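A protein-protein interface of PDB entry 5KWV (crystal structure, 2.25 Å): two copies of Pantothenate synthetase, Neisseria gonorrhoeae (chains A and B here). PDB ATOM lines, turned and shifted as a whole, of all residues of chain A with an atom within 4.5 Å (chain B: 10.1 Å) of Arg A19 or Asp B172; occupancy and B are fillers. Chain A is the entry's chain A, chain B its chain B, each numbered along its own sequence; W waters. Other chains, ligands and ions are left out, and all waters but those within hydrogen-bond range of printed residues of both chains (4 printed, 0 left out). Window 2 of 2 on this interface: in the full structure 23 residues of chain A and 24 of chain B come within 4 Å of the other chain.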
ATOM      1  N   ILE A  15      13.839   7.726  28.745  1.00  0.00           N
ATOM      2  CA  ILE A  15      14.136   8.115  27.369  1.00  0.00           C
ATOM      3  C   ILE A  15      15.329   9.059  27.333  1.00  0.00           C
ATOM      4  O   ILE A  15      16.205   8.944  26.465  1.00  0.00           O
ATOM      5  CB  ILE A  15      12.890   8.763  26.720  1.00  0.00           C
ATOM      6  CG1 ILE A  15      11.801   7.719  26.415  1.00  0.00           C
ATOM      7  CG2 ILE A  15      13.270   9.518  25.451  1.00  0.00           C
ATOM      8  CD1 ILE A  15      10.370   8.326  26.281  1.00  0.00           C
ATOM      9  N   ARG A  16      15.394   9.996  28.287  1.00  0.00           N
ATOM     10  CA  ARG A  16      16.466  10.984  28.283  1.00  0.00           C
ATOM     11  C   ARG A  16      17.831  10.330  28.469  1.00  0.00           C
ATOM     12  O   ARG A  16      18.803  10.717  27.811  1.00  0.00           O
ATOM     13  CB  ARG A  16      16.235  12.033  29.369  1.00  0.00           C
ATOM     14  CG  ARG A  16      16.242  13.452  28.823  1.00  0.00           C
ATOM     15  CD  ARG A  16      16.005  14.489  29.922  1.00  0.00           C
ATOM     16  NE  ARG A  16      17.170  14.606  30.792  1.00  0.00           N
ATOM     17  CZ  ARG A  16      18.135  15.510  30.635  1.00  0.00           C
ATOM     18  NH1 ARG A  16      18.065  16.390  29.644  1.00  0.00           N
ATOM     19  NH2 ARG A  16      19.168  15.538  31.469  1.00  0.00           N
ATOM     20  N   GLU A  17      17.936   9.364  29.391  1.00  0.00           N
ATOM     21  CA  GLU A  17      19.213   8.694  29.589  1.00  0.00           C
ATOM     22  C   GLU A  17      19.538   7.777  28.418  1.00  0.00           C
ATOM     23  O   GLU A  17      20.710   7.595  28.088  1.00  0.00           O
ATOM     24  CB  GLU A  17      19.216   7.901  30.891  1.00  0.00           C
ATOM     25  CG  GLU A  17      19.264   8.733  32.146  1.00  0.00           C
ATOM     26  CD  GLU A  17      19.028   7.894  33.382  1.00  0.00           C
ATOM     27  OE1 GLU A  17      18.105   7.043  33.356  1.00  0.00           O
ATOM     28  OE2 GLU A  17      19.781   8.067  34.366  1.00  0.00           O
ATOM     29  N   LEU A  18      18.523   7.185  27.785  1.00  0.00           N
ATOM     30  CA  LEU A  18      18.787   6.379  26.594  1.00  0.00           C
ATOM     31  C   LEU A  18      19.352   7.253  25.479  1.00  0.00           C
ATOM     32  O   LEU A  18      20.367   6.908  24.865  1.00  0.00           O
ATOM     33  CB  LEU A  18      17.511   5.663  26.139  1.00  0.00           C
ATOM     34  CG  LEU A  18      17.661   4.430  25.235  1.00  0.00           C
ATOM     35  CD1 LEU A  18      18.047   4.804  23.806  1.00  0.00           C
ATOM     36  CD2 LEU A  18      18.652   3.442  25.804  1.00  0.00           C
ATOM     37  N   ARG A  19      18.726   8.412  25.234  1.00  0.00           N
ATOM     38  CA  ARG A  19      19.211   9.319  24.197  1.00  0.00           C
ATOM     39  C   ARG A  19      20.636   9.793  24.481  1.00  0.00           C
ATOM     40  O   ARG A  19      21.468   9.854  23.566  1.00  0.00           O
ATOM     41  CB  ARG A  19      18.276  10.517  24.064  1.00  0.00           C
ATOM     42  CG  ARG A  19      16.855  10.188  23.625  1.00  0.00           C
ATOM     43  CD  ARG A  19      16.182  11.442  23.097  1.00  0.00           C
ATOM     44  NE  ARG A  19      14.779  11.215  22.760  1.00  0.00           N
ATOM     45  CZ  ARG A  19      14.375  10.649  21.628  1.00  0.00           C
ATOM     46  NH1 ARG A  19      15.275  10.248  20.731  1.00  0.00           N
ATOM     47  NH2 ARG A  19      13.079  10.484  21.382  1.00  0.00           N
ATOM     48  N   THR A  20      20.940  10.129  25.739  1.00  0.00           N
ATOM     49  CA  THR A  20      22.300  10.555  26.083  1.00  0.00           C
ATOM     50  C   THR A  20      23.324   9.453  25.822  1.00  0.00           C
ATOM     51  O   THR A  20      24.397   9.714  25.267  1.00  0.00           O
ATOM     52  CB  THR A  20      22.367  11.007  27.541  1.00  0.00           C
ATOM     53  OG1 THR A  20      21.490  12.123  27.722  1.00  0.00           O
ATOM     54  CG2 THR A  20      23.792  11.410  27.928  1.00  0.00           C
ATOM     55  N   TRP A  21      23.009   8.212  26.195  1.00  0.00           N
ATOM     56  CA  TRP A  21      23.951   7.123  25.946  1.00  0.00           C
ATOM     57  C   TRP A  21      24.133   6.865  24.449  1.00  0.00           C
ATOM     58  O   TRP A  21      25.240   6.553  23.995  1.00  0.00           O
ATOM     59  CB  TRP A  21      23.484   5.849  26.648  1.00  0.00           C
ATOM     60  CG  TRP A  21      24.225   4.659  26.138  1.00  0.00           C
ATOM     61  CD1 TRP A  21      25.429   4.178  26.591  1.00  0.00           C
ATOM     62  CD2 TRP A  21      23.837   3.810  25.050  1.00  0.00           C
ATOM     63  NE1 TRP A  21      25.798   3.079  25.856  1.00  0.00           N
ATOM     64  CE2 TRP A  21      24.843   2.832  24.904  1.00  0.00           C
ATOM     65  CE3 TRP A  21      22.737   3.783  24.186  1.00  0.00           C
ATOM     66  CZ2 TRP A  21      24.779   1.829  23.935  1.00  0.00           C
ATOM     67  CZ3 TRP A  21      22.680   2.788  23.216  1.00  0.00           C
ATOM     68  CH2 TRP A  21      23.696   1.823  23.103  1.00  0.00           C
ATOM     69  N   ARG A  22      23.053   6.973  23.674  1.00  0.00           N
ATOM     70  CA  ARG A  22      23.079   6.611  22.260  1.00  0.00           C
ATOM     71  C   ARG A  22      23.812   7.649  21.420  1.00  0.00           C
ATOM     72  O   ARG A  22      24.330   7.320  20.346  1.00  0.00           O
ATOM     73  CB  ARG A  22      21.643   6.441  21.747  1.00  0.00           C
ATOM     74  CG  ARG A  22      21.528   5.642  20.470  1.00  0.00           C
ATOM     75  CD  ARG A  22      21.507   6.507  19.231  1.00  0.00           C
ATOM     76  NE  ARG A  22      21.601   5.672  18.034  1.00  0.00           N
ATOM     77  CZ  ARG A  22      22.766   5.263  17.521  1.00  0.00           C
ATOM     78  NH1 ARG A  22      23.910   5.618  18.107  1.00  0.00           N
ATOM     79  NH2 ARG A  22      22.795   4.510  16.425  1.00  0.00           N
ATOM     80  N   GLU A  23      23.852   8.899  21.893  1.00  0.00           N
ATOM     81  CA  GLU A  23      24.421  10.002  21.126  1.00  0.00           C
ATOM     82  C   GLU A  23      25.890   9.778  20.780  1.00  0.00           C
ATOM     83  O   GLU A  23      26.309  10.029  19.644  1.00  0.00           O
ATOM     84  CB  GLU A  23      24.242  11.292  21.921  1.00  0.00           C
ATOM     85  CG  GLU A  23      24.413  12.574  21.133  1.00  0.00           C
ATOM     86  CD  GLU A  23      24.147  13.816  21.983  1.00  0.00           C
ATOM     87  OE1 GLU A  23      24.258  14.941  21.449  1.00  0.00           O
ATOM     88  OE2 GLU A  23      23.813  13.669  23.183  1.00  0.00           O
ATOM     89  N   ASN A 142      12.077   5.624  17.291  1.00  0.00           N
ATOM     90  CA  ASN A 142      12.388   7.049  17.440  1.00  0.00           C
ATOM     91  C   ASN A 142      13.156   7.364  18.712  1.00  0.00           C
ATOM     92  O   ASN A 142      13.780   8.437  18.789  1.00  0.00           O
ATOM     93  CB  ASN A 142      11.108   7.885  17.431  1.00  0.00           C
ATOM     94  CG  ASN A 142      10.618   8.168  16.049  1.00  0.00           C
ATOM     95  OD1 ASN A 142      11.387   8.099  15.090  1.00  0.00           O
ATOM     96  ND2 ASN A 142       9.323   8.521  15.927  1.00  0.00           N
ATOM     97  N   ILE A 143      13.096   6.474  19.709  1.00  0.00           N
ATOM     98  CA  ILE A 143      13.852   6.623  20.949  1.00  0.00           C
ATOM     99  C   ILE A 143      15.277   6.098  20.788  1.00  0.00           C
ATOM    100  O   ILE A 143      16.251   6.773  21.133  1.00  0.00           O
ATOM    101  CB  ILE A 143      13.125   5.879  22.089  1.00  0.00           C
ATOM    102  CG1 ILE A 143      11.810   6.567  22.484  1.00  0.00           C
ATOM    103  CG2 ILE A 143      14.045   5.677  23.277  1.00  0.00           C
ATOM    104  CD1 ILE A 143      10.913   5.646  23.321  1.00  0.00           C
ATOM    105  N   ARG B  22      23.039  14.820   5.182  1.00  0.00           N
ATOM    106  CA  ARG B  22      22.684  15.186   6.555  1.00  0.00           C
ATOM    107  C   ARG B  22      23.630  14.569   7.578  1.00  0.00           C
ATOM    108  O   ARG B  22      23.896  15.181   8.618  1.00  0.00           O
ATOM    109  CB  ARG B  22      21.232  14.775   6.845  1.00  0.00           C
ATOM    110  CG  ARG B  22      20.606  15.438   8.056  1.00  0.00           C
ATOM    111  CD  ARG B  22      20.731  14.578   9.303  1.00  0.00           C
ATOM    112  NE  ARG B  22      20.238  15.262  10.498  1.00  0.00           N
ATOM    113  CZ  ARG B  22      20.962  16.082  11.248  1.00  0.00           C
ATOM    114  NH1 ARG B  22      20.421  16.653  12.313  1.00  0.00           N
ATOM    115  NH2 ARG B  22      22.226  16.330  10.937  1.00  0.00           N
ATOM    116  N   LYS B  27      23.559  20.508  13.660  1.00  0.00           N
ATOM    117  CA  LYS B  27      22.166  20.812  13.935  1.00  0.00           C
ATOM    118  C   LYS B  27      21.450  21.172  12.640  1.00  0.00           C
ATOM    119  O   LYS B  27      21.994  21.868  11.781  1.00  0.00           O
ATOM    120  CB  LYS B  27      22.086  21.957  14.950  1.00  0.00           C
ATOM    121  CG  LYS B  27      20.810  21.999  15.783  1.00  0.00           C
ATOM    122  CD  LYS B  27      20.869  23.123  16.815  1.00  0.00           C
ATOM    123  CE  LYS B  27      19.527  23.318  17.508  1.00  0.00           C
ATOM    124  NZ  LYS B  27      19.476  24.591  18.282  1.00  0.00           N
ATOM    125  N   VAL B  28      20.219  20.696  12.493  1.00  0.00           N
ATOM    126  CA  VAL B  28      19.424  20.981  11.305  1.00  0.00           C
ATOM    127  C   VAL B  28      18.068  21.520  11.745  1.00  0.00           C
ATOM    128  O   VAL B  28      17.397  20.925  12.600  1.00  0.00           O
ATOM    129  CB  VAL B  28      19.249  19.738  10.410  1.00  0.00           C
ATOM    130  CG1 VAL B  28      18.147  19.973   9.383  1.00  0.00           C
ATOM    131  CG2 VAL B  28      20.557  19.378   9.709  1.00  0.00           C
ATOM    132  N   PHE B 141      10.128  13.708   8.698  1.00  0.00           N
ATOM    133  CA  PHE B 141      10.936  13.706   9.915  1.00  0.00           C
ATOM    134  C   PHE B 141      11.965  12.573   9.894  1.00  0.00           C
ATOM    135  O   PHE B 141      13.099  12.748  10.348  1.00  0.00           O
ATOM    136  CB  PHE B 141      10.033  13.593  11.156  1.00  0.00           C
ATOM    137  CG  PHE B 141       9.373  14.914  11.581  1.00  0.00           C
ATOM    138  CD1 PHE B 141       9.713  16.115  10.979  1.00  0.00           C
ATOM    139  CD2 PHE B 141       8.433  14.936  12.605  1.00  0.00           C
ATOM    140  CE1 PHE B 141       9.122  17.316  11.390  1.00  0.00           C
ATOM    141  CE2 PHE B 141       7.851  16.130  13.020  1.00  0.00           C
ATOM    142  CZ  PHE B 141       8.180  17.315  12.404  1.00  0.00           C
ATOM    143  N   ASN B 142      11.552  11.383   9.439  1.00  0.00           N
ATOM    144  CA  ASN B 142      12.438  10.234   9.356  1.00  0.00           C
ATOM    145  C   ASN B 142      13.432  10.337   8.215  1.00  0.00           C
ATOM    146  O   ASN B 142      14.397   9.587   8.217  1.00  0.00           O
ATOM    147  CB  ASN B 142      11.641   8.946   9.188  1.00  0.00           C
ATOM    148  CG  ASN B 142      11.099   8.444  10.492  1.00  0.00           C
ATOM    149  OD1 ASN B 142      11.623   8.782  11.554  1.00  0.00           O
ATOM    150  ND2 ASN B 142      10.016   7.652  10.430  1.00  0.00           N
ATOM    151  N   VAL B 144      14.726  13.570   7.042  1.00  0.00           N
ATOM    152  CA  VAL B 144      15.636  14.676   7.329  1.00  0.00           C
ATOM    153  C   VAL B 144      16.343  14.485   8.661  1.00  0.00           C
ATOM    154  O   VAL B 144      17.470  14.953   8.837  1.00  0.00           O
ATOM    155  CB  VAL B 144      14.874  16.014   7.307  1.00  0.00           C
ATOM    156  CG1 VAL B 144      15.774  17.164   7.737  1.00  0.00           C
ATOM    157  CG2 VAL B 144      14.284  16.281   5.928  1.00  0.00           C
ATOM    158  N   LEU B 145      15.719  13.796   9.607  1.00  0.00           N
ATOM    159  CA  LEU B 145      16.216  13.710  10.975  1.00  0.00           C
ATOM    160  C   LEU B 145      16.587  15.093  11.515  1.00  0.00           C
ATOM    161  O   LEU B 145      17.730  15.320  11.924  1.00  0.00           O
ATOM    162  CB  LEU B 145      17.399  12.756  11.072  1.00  0.00           C
ATOM    163  CG  LEU B 145      17.086  11.290  10.724  1.00  0.00           C
ATOM    164  CD1 LEU B 145      18.356  10.429  10.659  1.00  0.00           C
ATOM    165  CD2 LEU B 145      16.058  10.699  11.716  1.00  0.00           C
ATOM    166  N   PRO B 146      15.641  16.029  11.559  1.00  0.00           N
ATOM    167  CA  PRO B 146      15.965  17.382  12.011  1.00  0.00           C
ATOM    168  C   PRO B 146      16.025  17.471  13.528  1.00  0.00           C
ATOM    169  O   PRO B 146      15.560  16.591  14.255  1.00  0.00           O
ATOM    170  CB  PRO B 146      14.806  18.212  11.466  1.00  0.00           C
ATOM    171  CG  PRO B 146      13.630  17.272  11.584  1.00  0.00           C
ATOM    172  CD  PRO B 146      14.194  15.876  11.308  1.00  0.00           C
ATOM    173  N   ASP B 147      16.662  18.541  13.996  1.00  0.00           N
ATOM    174  CA  ASP B 147      16.626  18.883  15.412  1.00  0.00           C
ATOM    175  C   ASP B 147      15.505  19.860  15.740  1.00  0.00           C
ATOM    176  O   ASP B 147      14.988  19.848  16.861  1.00  0.00           O
ATOM    177  CB  ASP B 147      17.973  19.481  15.838  1.00  0.00           C
ATOM    178  CG  ASP B 147      19.130  18.524  15.596  1.00  0.00           C
ATOM    179  OD1 ASP B 147      19.859  18.684  14.596  1.00  0.00           O
ATOM    180  OD2 ASP B 147      19.291  17.588  16.403  1.00  0.00           O
ATOM    181  N   VAL B 148      15.118  20.690  14.774  1.00  0.00           N
ATOM    182  CA  VAL B 148      14.134  21.753  14.942  1.00  0.00           C
ATOM    183  C   VAL B 148      13.291  21.790  13.672  1.00  0.00           C
ATOM    184  O   VAL B 148      13.818  21.614  12.568  1.00  0.00           O
ATOM    185  CB  VAL B 148      14.815  23.119  15.192  1.00  0.00           C
ATOM    186  CG1 VAL B 148      13.791  24.228  15.252  1.00  0.00           C
ATOM    187  CG2 VAL B 148      15.658  23.093  16.461  1.00  0.00           C
ATOM    188  N   ALA B 149      11.980  21.989  13.825  1.00  0.00           N
ATOM    189  CA  ALA B 149      11.082  22.094  12.678  1.00  0.00           C
ATOM    190  C   ALA B 149      10.101  23.227  12.917  1.00  0.00           C
ATOM    191  O   ALA B 149       9.473  23.277  13.976  1.00  0.00           O
ATOM    192  CB  ALA B 149      10.328  20.778  12.433  1.00  0.00           C
ATOM    193  N   ILE B 162       0.734  18.235  14.490  1.00  0.00           N
ATOM    194  CA  ILE B 162       2.156  17.930  14.383  1.00  0.00           C
ATOM    195  C   ILE B 162       2.801  17.902  15.763  1.00  0.00           C
ATOM    196  O   ILE B 162       3.622  17.032  16.047  1.00  0.00           O
ATOM    197  CB  ILE B 162       2.834  18.931  13.432  1.00  0.00           C
ATOM    198  CG1 ILE B 162       2.393  18.629  11.996  1.00  0.00           C
ATOM    199  CG2 ILE B 162       4.378  18.887  13.568  1.00  0.00           C
ATOM    200  CD1 ILE B 162       2.678  19.759  11.043  1.00  0.00           C
ATOM    201  N   LYS B 163       2.417  18.826  16.656  1.00  0.00           N
ATOM    202  CA  LYS B 163       2.872  18.724  18.039  1.00  0.00           C
ATOM    203  C   LYS B 163       2.441  17.400  18.656  1.00  0.00           C
ATOM    204  O   LYS B 163       3.237  16.729  19.323  1.00  0.00           O
ATOM    205  CB  LYS B 163       2.339  19.891  18.883  1.00  0.00           C
ATOM    206  CG  LYS B 163       2.967  21.252  18.610  1.00  0.00           C
ATOM    207  CD  LYS B 163       2.749  22.196  19.801  1.00  0.00           C
ATOM    208  CE  LYS B 163       3.408  23.566  19.598  1.00  0.00           C
ATOM    209  NZ  LYS B 163       3.254  24.480  20.782  1.00  0.00           N
ATOM    210  N   LEU B 165       1.655  14.412  17.210  1.00  0.00           N
ATOM    211  CA  LEU B 165       2.361  13.230  16.711  1.00  0.00           C
ATOM    212  C   LEU B 165       3.807  13.203  17.210  1.00  0.00           C
ATOM    213  O   LEU B 165       4.352  12.137  17.507  1.00  0.00           O
ATOM    214  CB  LEU B 165       2.317  13.188  15.183  1.00  0.00           C
ATOM    215  CG  LEU B 165       3.176  14.113  14.315  1.00  0.00           C
ATOM    216  CD1 LEU B 165       4.591  13.562  14.116  1.00  0.00           C
ATOM    217  CD2 LEU B 165       2.513  14.276  12.953  1.00  0.00           C
ATOM    218  N   THR B 166       4.439  14.375  17.296  1.00  0.00           N
ATOM    219  CA  THR B 166       5.803  14.470  17.799  1.00  0.00           C
ATOM    220  C   THR B 166       5.908  13.921  19.224  1.00  0.00           C
ATOM    221  O   THR B 166       6.786  13.095  19.518  1.00  0.00           O
ATOM    222  CB  THR B 166       6.259  15.929  17.709  1.00  0.00           C
ATOM    223  OG1 THR B 166       6.300  16.323  16.325  1.00  0.00           O
ATOM    224  CG2 THR B 166       7.632  16.133  18.328  1.00  0.00           C
ATOM    225  N   GLU B 167       5.000  14.344  20.118  1.00  0.00           N
ATOM    226  CA  GLU B 167       4.990  13.823  21.484  1.00  0.00           C
ATOM    227  C   GLU B 167       4.671  12.332  21.510  1.00  0.00           C
ATOM    228  O   GLU B 167       5.370  11.546  22.153  1.00  0.00           O
ATOM    229  CB  GLU B 167       3.963  14.560  22.338  1.00  0.00           C
ATOM    230  CG  GLU B 167       4.169  16.047  22.513  1.00  0.00           C
ATOM    231  CD  GLU B 167       3.022  16.692  23.297  1.00  0.00           C
ATOM    232  OE1 GLU B 167       2.182  15.947  23.867  1.00  0.00           O
ATOM    233  OE2 GLU B 167       2.958  17.942  23.335  1.00  0.00           O
ATOM    234  N   ASP B 168       3.580  11.935  20.859  1.00  0.00           N
ATOM    235  CA  ASP B 168       3.103  10.561  20.998  1.00  0.00           C
ATOM    236  C   ASP B 168       4.027   9.546  20.323  1.00  0.00           C
ATOM    237  O   ASP B 168       4.032   8.375  20.709  1.00  0.00           O
ATOM    238  CB  ASP B 168       1.697  10.424  20.418  1.00  0.00           C
ATOM    239  CG  ASP B 168       0.615  10.860  21.384  1.00  0.00           C
ATOM    240  OD1 ASP B 168       0.930  11.517  22.406  1.00  0.00           O
ATOM    241  OD2 ASP B 168      -0.562  10.556  21.100  1.00  0.00           O
ATOM    242  N   LEU B 169       4.767   9.941  19.288  1.00  0.00           N
ATOM    243  CA  LEU B 169       5.674   9.007  18.624  1.00  0.00           C
ATOM    244  C   LEU B 169       7.135   9.217  19.024  1.00  0.00           C
ATOM    245  O   LEU B 169       8.020   8.582  18.444  1.00  0.00           O
ATOM    246  CB  LEU B 169       5.526   9.116  17.103  1.00  0.00           C
ATOM    247  CG  LEU B 169       4.095   8.878  16.566  1.00  0.00           C
ATOM    248  CD1 LEU B 169       4.007   9.127  15.047  1.00  0.00           C
ATOM    249  CD2 LEU B 169       3.583   7.482  16.933  1.00  0.00           C
ATOM    250  N   ASN B 170       7.403  10.089  19.997  1.00  0.00           N
ATOM    251  CA  ASN B 170       8.757  10.320  20.523  1.00  0.00           C
ATOM    252  C   ASN B 170       9.751  10.747  19.439  1.00  0.00           C
ATOM    253  O   ASN B 170      10.908  10.308  19.422  1.00  0.00           O
ATOM    254  CB  ASN B 170       9.285   9.092  21.272  1.00  0.00           C
ATOM    255  CG  ASN B 170       8.384   8.677  22.420  1.00  0.00           C
ATOM    256  OD1 ASN B 170       7.592   7.743  22.290  1.00  0.00           O
ATOM    257  ND2 ASN B 170       8.480   9.397  23.545  1.00  0.00           N
ATOM    258  N   PHE B 171       9.302  11.590  18.508  1.00  0.00           N
ATOM    259  CA  PHE B 171      10.237  12.272  17.620  1.00  0.00           C
ATOM    260  C   PHE B 171      11.022  13.282  18.443  1.00  0.00           C
ATOM    261  O   PHE B 171      10.429  14.172  19.067  1.00  0.00           O
ATOM    262  CB  PHE B 171       9.518  12.983  16.477  1.00  0.00           C
ATOM    263  CG  PHE B 171       9.109  12.079  15.335  1.00  0.00           C
ATOM    264  CD1 PHE B 171      10.065  11.568  14.445  1.00  0.00           C
ATOM    265  CD2 PHE B 171       7.762  11.797  15.110  1.00  0.00           C
ATOM    266  CE1 PHE B 171       9.678  10.751  13.369  1.00  0.00           C
ATOM    267  CE2 PHE B 171       7.361  10.976  14.045  1.00  0.00           C
ATOM    268  CZ  PHE B 171       8.325  10.448  13.174  1.00  0.00           C
ATOM    269  N   ASP B 172      12.355  13.166  18.433  1.00  0.00           N
ATOM    270  CA  ASP B 172      13.199  14.068  19.215  1.00  0.00           C
ATOM    271  C   ASP B 172      13.418  15.367  18.439  1.00  0.00           C
ATOM    272  O   ASP B 172      14.526  15.711  18.024  1.00  0.00           O
ATOM    273  CB  ASP B 172      14.521  13.400  19.557  1.00  0.00           C
ATOM    274  CG  ASP B 172      15.349  14.231  20.507  1.00  0.00           C
ATOM    275  OD1 ASP B 172      14.758  15.055  21.217  1.00  0.00           O
ATOM    276  OD2 ASP B 172      16.585  14.065  20.551  1.00  0.00           O
ATOM    277  N   ILE B 173      12.326  16.102  18.233  1.00  0.00           N
ATOM    278  CA  ILE B 173      12.345  17.285  17.374  1.00  0.00           C
ATOM    279  C   ILE B 173      11.657  18.440  18.096  1.00  0.00           C
ATOM    280  O   ILE B 173      10.532  18.292  18.587  1.00  0.00           O
ATOM    281  CB  ILE B 173      11.656  17.019  16.019  1.00  0.00           C
ATOM    282  CG1 ILE B 173      12.310  15.851  15.283  1.00  0.00           C
ATOM    283  CG2 ILE B 173      11.707  18.258  15.154  1.00  0.00           C
ATOM    284  CD1 ILE B 173      11.523  15.393  14.084  1.00  0.00           C
ATOM    285  N   GLU B 174      12.311  19.594  18.124  1.00  0.00           N
ATOM    286  CA  GLU B 174      11.697  20.783  18.695  1.00  0.00           C
ATOM    287  C   GLU B 174      10.788  21.417  17.651  1.00  0.00           C
ATOM    288  O   GLU B 174      11.251  21.814  16.574  1.00  0.00           O
ATOM    289  CB  GLU B 174      12.761  21.776  19.163  1.00  0.00           C
ATOM    290  CG  GLU B 174      12.177  23.019  19.839  1.00  0.00           C
ATOM    291  CD  GLU B 174      13.234  24.065  20.194  1.00  0.00           C
ATOM    292  OE1 GLU B 174      12.841  25.184  20.601  1.00  0.00           O
ATOM    293  OE2 GLU B 174      14.448  23.770  20.072  1.00  0.00           O
ATOM    294  N   ILE B 175       9.500  21.500  17.962  1.00  0.00           N
ATOM    295  CA  ILE B 175       8.518  22.079  17.052  1.00  0.00           C
ATOM    296  C   ILE B 175       8.346  23.549  17.429  1.00  0.00           C
ATOM    297  O   ILE B 175       7.976  23.872  18.561  1.00  0.00           O
ATOM    298  CB  ILE B 175       7.181  21.324  17.107  1.00  0.00           C
ATOM    299  CG1 ILE B 175       7.395  19.815  16.926  1.00  0.00           C
ATOM    300  CG2 ILE B 175       6.259  21.826  16.019  1.00  0.00           C
ATOM    301  CD1 ILE B 175       7.906  19.418  15.551  1.00  0.00           C
HETATM  302  O   HOH W   1      10.822  11.522  23.228  1.00  0.00           O
HETATM  303  O   HOH W   2      13.580  10.736  17.197  1.00  0.00           O
HETATM  304  O   HOH W   3      13.394   9.835  14.299  1.00  0.00           O
HETATM  305  O   HOH W   4      13.860   7.817  12.773  1.00  0.00           O
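The backbone carbonyl oxygen of Asn B170 is in hydrogen-bond range of the guanidinium group of Arg A19 (2.9 Å). O of Leu B169 is in hydrogen-bond range of ND2 of Asn A142 (2.8 Å). The backbone carbonyl oxygen of Asn A142 lies close to the backbone carbonyl oxygen of Asn B170, at 3.5 Å.
Of the 11 printed residues of chain A, 4 touch a printed residue of chain B. Of the 24 printed residues of chain B, 5 touch a printed residue of chain A. Hydrophobic or aromatic side chains of chain B that line the printed part of chain A: Phe B171. Along chain B the printed residues that touch a printed residue of chain A span positions 142 to 172. Among the printed residues, 8 pairs touch across the chains. Among the printed residues, no Asp or Glu carboxylate lies within 4 Å of a Lys or Arg side-chain nitrogen of the other chain.
Water W4 bridges OD1 of Asn B142 (2.7 Å) and OD1 of Asn A142 (3.4 Å). Water W3 bridges the side-chain amide oxygen (OD1) of Asn A142 (2.8 Å) and the side-chain amide oxygen (OD1) of Asn B142 (3.4 Å). Water W2 bridges O of Asn A142 and N of Asp B172. Water W1 lies within hydrogen-bond range of the guanidinium group of Arg A19 (3.1 Å) and the side-chain amide nitrogen of Asn B170 (3.2 Å).
NH1 of Arg A19 lies within hydrogen-bond range of O of Asn A142 (3.0 Å). The backbone NH (N) of Phe B171 sits at hydrogen-bond distance from the backbone carbonyl oxygen (O) of Thr B166 (3.1 Å).
Arg A19 touches just these residues of chain B: Asn B170 and Asp B172. Printed residues of chain A within 4 Å of Asp B172: Arg A19. No residue of chain B comes within 4 Å of Thr A20. Of chain B, only Asn B170 comes within 4 Å of Ile A143. Of the printed residues of chain A, Asn B142 touches Asn A142. Printed residues of chain A within 4 Å of Phe B171: Asn A142. Printed residues of chain A within 4 Å of Asn B170: Ile A15, Arg A19, Asn A142 and Ile A143. Of the printed residues of chain B, Ile A15 touches Asn B170 (3.5 Å). The nearest printed residue of chain A that does not touch Asp B172 is Asn A142 (5.0 Å). The nearest printed residue of chain B that does not touch Ile A15 is Asp B172 (7.1 Å).
Ile A15 touches Asn B170. Asp B172 touches Arg A19 (CB to CZ, 3.4 Å). Asn A142 touches Asn B142. Phe B171 touches Asn A142 (CE1 to ND2, 3.4 Å). Asn B170 touches Ile A143 (CB to CG1, 3.8 Å).
Asn B142 touches its own counterpart, Asn A142.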
